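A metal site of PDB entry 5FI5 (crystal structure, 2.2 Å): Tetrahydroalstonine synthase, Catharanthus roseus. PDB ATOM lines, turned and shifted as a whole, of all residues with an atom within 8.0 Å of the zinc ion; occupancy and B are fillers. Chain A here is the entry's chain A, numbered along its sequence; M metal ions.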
ATOM      1  N   GLU A 106      22.711   2.163  14.614  1.00  0.00           N
ATOM      2  CA  GLU A 106      24.178   2.080  14.515  1.00  0.00           C
ATOM      3  C   GLU A 106      24.753   3.194  13.658  1.00  0.00           C
ATOM      4  O   GLU A 106      24.089   3.722  12.757  1.00  0.00           O
ATOM      5  CB  GLU A 106      24.639   0.705  13.996  1.00  0.00           C
ATOM      6  CG  GLU A 106      24.148   0.326  12.603  1.00  0.00           C
ATOM      7  CD  GLU A 106      24.649  -1.045  12.164  1.00  0.00           C
ATOM      8  OE1 GLU A 106      25.881  -1.205  12.013  1.00  0.00           O
ATOM      9  OE2 GLU A 106      23.821  -1.959  11.990  1.00  0.00           O
ATOM     10  N   THR A 107      25.997   3.560  13.967  1.00  0.00           N
ATOM     11  CA  THR A 107      26.768   4.525  13.171  1.00  0.00           C
ATOM     12  C   THR A 107      28.224   4.060  13.147  1.00  0.00           C
ATOM     13  O   THR A 107      28.561   3.071  13.777  1.00  0.00           O
ATOM     14  CB  THR A 107      26.691   5.949  13.748  1.00  0.00           C
ATOM     15  OG1 THR A 107      27.322   5.966  15.029  1.00  0.00           O
ATOM     16  CG2 THR A 107      25.255   6.401  13.903  1.00  0.00           C
ATOM     17  N   CYS A 108      29.064   4.758  12.396  1.00  0.00           N
ATOM     18  CA  CYS A 108      30.451   4.318  12.201  1.00  0.00           C
ATOM     19  C   CYS A 108      31.297   4.469  13.473  1.00  0.00           C
ATOM     20  O   CYS A 108      32.201   3.681  13.689  1.00  0.00           O
ATOM     21  CB  CYS A 108      31.102   5.074  11.012  1.00  0.00           C
ATOM     22  SG  CYS A 108      31.795   6.706  11.394  1.00  0.00           S
ATOM     23  N   GLY A 109      31.018   5.494  14.298  1.00  0.00           N
ATOM     24  CA  GLY A 109      31.746   5.737  15.554  1.00  0.00           C
ATOM     25  C   GLY A 109      33.024   6.572  15.460  1.00  0.00           C
ATOM     26  O   GLY A 109      33.486   7.084  16.492  1.00  0.00           O
ATOM     27  N   LYS A 110      33.604   6.690  14.259  1.00  0.00           N
ATOM     28  CA  LYS A 110      34.918   7.356  14.024  1.00  0.00           C
ATOM     29  C   LYS A 110      34.819   8.811  13.488  1.00  0.00           C
ATOM     30  O   LYS A 110      35.677   9.646  13.793  1.00  0.00           O
ATOM     31  CB  LYS A 110      35.766   6.524  13.037  1.00  0.00           C
ATOM     32  CG  LYS A 110      35.952   5.052  13.426  1.00  0.00           C
ATOM     33  N   CYS A 111      33.778   9.106  12.700  1.00  0.00           N
ATOM     34  CA  CYS A 111      33.669  10.414  12.024  1.00  0.00           C
ATOM     35  C   CYS A 111      33.473  11.597  12.985  1.00  0.00           C
ATOM     36  O   CYS A 111      33.180  11.407  14.175  1.00  0.00           O
ATOM     37  CB  CYS A 111      32.521  10.368  11.021  1.00  0.00           C
ATOM     38  SG  CYS A 111      30.926  10.338  11.839  1.00  0.00           S
ATOM     39  N   GLU A 112      33.571  12.818  12.450  1.00  0.00           N
ATOM     40  CA  GLU A 112      33.351  14.046  13.226  1.00  0.00           C
ATOM     41  C   GLU A 112      31.937  14.100  13.847  1.00  0.00           C
ATOM     42  O   GLU A 112      31.747  14.527  14.981  1.00  0.00           O
ATOM     43  CB  GLU A 112      33.561  15.267  12.337  1.00  0.00           C
ATOM     44  CG  GLU A 112      33.431  16.637  13.007  1.00  0.00           C
ATOM     45  CD  GLU A 112      33.516  17.810  12.028  1.00  0.00           C
ATOM     46  OE1 GLU A 112      34.072  17.675  10.918  1.00  0.00           O
ATOM     47  OE2 GLU A 112      33.051  18.908  12.371  1.00  0.00           O
ATOM     48  N   MET A 113      30.945  13.684  13.076  1.00  0.00           N
ATOM     49  CA  MET A 113      29.551  13.680  13.557  1.00  0.00           C
ATOM     50  C   MET A 113      29.363  12.647  14.690  1.00  0.00           C
ATOM     51  O   MET A 113      28.682  12.925  15.700  1.00  0.00           O
ATOM     52  CB  MET A 113      28.558  13.483  12.391  1.00  0.00           C
ATOM     53  CG  MET A 113      28.701  14.509  11.251  1.00  0.00           C
ATOM     54  SD  MET A 113      28.444  16.197  11.830  1.00  0.00           S
ATOM     55  CE  MET A 113      29.780  17.097  11.041  1.00  0.00           C
ATOM     56  N   CYS A 114      30.028  11.497  14.565  1.00  0.00           N
ATOM     57  CA  CYS A 114      29.993  10.479  15.596  1.00  0.00           C
ATOM     58  C   CYS A 114      30.682  10.933  16.888  1.00  0.00           C
ATOM     59  O   CYS A 114      30.099  10.844  17.979  1.00  0.00           O
ATOM     60  CB  CYS A 114      30.562   9.174  15.077  1.00  0.00           C
ATOM     61  SG  CYS A 114      29.375   8.324  14.026  1.00  0.00           S
ATOM     62  N   THR A 115      31.902  11.466  16.779  1.00  0.00           N
ATOM     63  CA  THR A 115      32.669  11.838  17.987  1.00  0.00           C
ATOM     64  C   THR A 115      32.095  13.076  18.663  1.00  0.00           C
ATOM     65  O   THR A 115      32.274  13.242  19.867  1.00  0.00           O
ATOM     66  CB  THR A 115      34.188  12.009  17.729  1.00  0.00           C
ATOM     67  OG1 THR A 115      34.452  13.160  16.922  1.00  0.00           O
ATOM     68  CG2 THR A 115      34.785  10.755  17.078  1.00  0.00           C
ATOM     69  N   VAL A 118      26.616  14.021  17.474  1.00  0.00           N
ATOM     70  CA  VAL A 118      25.553  14.366  16.535  1.00  0.00           C
ATOM     71  C   VAL A 118      25.520  13.273  15.462  1.00  0.00           C
ATOM     72  O   VAL A 118      25.462  13.527  14.259  1.00  0.00           O
ATOM     73  CB  VAL A 118      25.655  15.826  16.018  1.00  0.00           C
ATOM     74  CG1 VAL A 118      25.494  16.807  17.188  1.00  0.00           C
ATOM     75  CG2 VAL A 118      26.975  16.104  15.311  1.00  0.00           C
ATOM     76  N   GLU A 119      25.536  12.047  15.954  1.00  0.00           N
ATOM     77  CA  GLU A 119      25.734  10.848  15.132  1.00  0.00           C
ATOM     78  C   GLU A 119      24.544  10.495  14.266  1.00  0.00           C
ATOM     79  O   GLU A 119      24.630   9.652  13.374  1.00  0.00           O
ATOM     80  CB  GLU A 119      26.159   9.663  15.999  1.00  0.00           C
ATOM     81  CG  GLU A 119      25.093   8.923  16.794  1.00  0.00           C
ATOM     82  CD  GLU A 119      24.467   9.721  17.923  1.00  0.00           C
ATOM     83  OE1 GLU A 119      25.169  10.541  18.603  1.00  0.00           O
ATOM     84  OE2 GLU A 119      23.252   9.531  18.123  1.00  0.00           O
ATOM     85  N   ASN A 120      23.411  11.152  14.501  1.00  0.00           N
ATOM     86  CA  ASN A 120      22.297  11.083  13.548  1.00  0.00           C
ATOM     87  C   ASN A 120      22.659  11.607  12.162  1.00  0.00           C
ATOM     88  O   ASN A 120      22.015  11.222  11.185  1.00  0.00           O
ATOM     89  CB  ASN A 120      21.047  11.798  14.092  1.00  0.00           C
ATOM     90  CG  ASN A 120      21.252  13.296  14.306  1.00  0.00           C
ATOM     91  OD1 ASN A 120      22.150  13.718  15.032  1.00  0.00           O
ATOM     92  ND2 ASN A 120      20.364  14.116  13.723  1.00  0.00           N
ATOM     93  N   TYR A 121      23.682  12.446  12.083  1.00  0.00           N
ATOM     94  CA  TYR A 121      24.216  12.907  10.810  1.00  0.00           C
ATOM     95  C   TYR A 121      25.432  12.122  10.291  1.00  0.00           C
ATOM     96  O   TYR A 121      26.072  12.561   9.343  1.00  0.00           O
ATOM     97  CB  TYR A 121      24.513  14.402  10.926  1.00  0.00           C
ATOM     98  CG  TYR A 121      23.254  15.227  11.069  1.00  0.00           C
ATOM     99  CD1 TYR A 121      22.340  15.292  10.040  1.00  0.00           C
ATOM    100  CD2 TYR A 121      22.979  15.912  12.250  1.00  0.00           C
ATOM    101  CE1 TYR A 121      21.185  16.029  10.165  1.00  0.00           C
ATOM    102  CE2 TYR A 121      21.820  16.643  12.391  1.00  0.00           C
ATOM    103  CZ  TYR A 121      20.931  16.707  11.343  1.00  0.00           C
ATOM    104  OH  TYR A 121      19.763  17.437  11.487  1.00  0.00           O
ATOM    105  N   CYS A 122      25.721  10.956  10.869  1.00  0.00           N
ATOM    106  CA  CYS A 122      26.802  10.102  10.369  1.00  0.00           C
ATOM    107  C   CYS A 122      26.488   9.700   8.947  1.00  0.00           C
ATOM    108  O   CYS A 122      25.383   9.185   8.715  1.00  0.00           O
ATOM    109  CB  CYS A 122      26.928   8.804  11.201  1.00  0.00           C
ATOM    110  SG  CYS A 122      28.139   7.597  10.563  1.00  0.00           S
ATOM    111  N   PRO A 123      27.453   9.868   8.005  1.00  0.00           N
ATOM    112  CA  PRO A 123      27.239   9.402   6.624  1.00  0.00           C
ATOM    113  C   PRO A 123      26.885   7.908   6.501  1.00  0.00           C
ATOM    114  O   PRO A 123      26.226   7.525   5.539  1.00  0.00           O
ATOM    115  CB  PRO A 123      28.561   9.698   5.929  1.00  0.00           C
ATOM    116  CG  PRO A 123      29.175  10.801   6.715  1.00  0.00           C
ATOM    117  CD  PRO A 123      28.725  10.598   8.137  1.00  0.00           C
ATOM    118  N   GLU A 124      27.318   7.099   7.452  1.00  0.00           N
ATOM    119  CA  GLU A 124      27.099   5.640   7.410  1.00  0.00           C
ATOM    120  C   GLU A 124      26.079   5.155   8.451  1.00  0.00           C
ATOM    121  O   GLU A 124      26.083   3.983   8.822  1.00  0.00           O
ATOM    122  CB  GLU A 124      28.459   4.918   7.570  1.00  0.00           C
ATOM    123  CG  GLU A 124      29.357   5.056   6.334  1.00  0.00           C
ATOM    124  CD  GLU A 124      30.811   4.756   6.621  1.00  0.00           C
ATOM    125  OE1 GLU A 124      31.415   5.450   7.448  1.00  0.00           O
ATOM    126  OE2 GLU A 124      31.371   3.826   6.001  1.00  0.00           O
ATOM    127  N   ALA A 125      25.194   6.042   8.885  1.00  0.00           N
ATOM    128  CA  ALA A 125      24.160   5.706   9.835  1.00  0.00           C
ATOM    129  C   ALA A 125      23.318   4.556   9.310  1.00  0.00           C
ATOM    130  O   ALA A 125      22.934   4.545   8.140  1.00  0.00           O
ATOM    131  CB  ALA A 125      23.274   6.911  10.138  1.00  0.00           C
HETATM  132 ZN    ZN M   1      30.031   8.201  11.776  1.00  0.00          ZN
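The zinc ion is bound by the side-chain sulfur (SG) of Cys 111 (2.3 Å), the side-chain sulfur (SG) of Cys 122 (2.3 Å), the side-chain sulfur (SG) of Cys 108 (2.3 Å) and the side-chain sulfur (SG) of Cys 114 (2.3 Å).
Residues that only touch the zinc ion: Gly 109. Of the 18 residues printed, 5 come within 4 Å of the zinc ion. The nearest printed residue that does not touch the zinc ion is Thr 107 (4.5 Å).
SG of Cys 122 lies close to N of Ala 125. The backbone NH (N) of Lys 110 sits close to the side-chain sulfur (SG) of Cys 108 (3.4 Å). The backbone NH (N) of Gly 109 sits close to the side-chain sulfur (SG) of Cys 114 (3.3 Å). O of Cys 111 sits close to OG1 of Thr 115. The side-chain sulfur (SG) of Cys 111 lies close to the backbone NH (N) of Met 113. The side-chain sulfur (SG) of Cys 114 lies close to the side-chain hydroxyl (OG1) of Thr 107, 3.3 Å away. The side-chain sulfur (SG) of Cys 122 lies close to the backbone NH (N) of Glu 124, 3.3 Å away.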
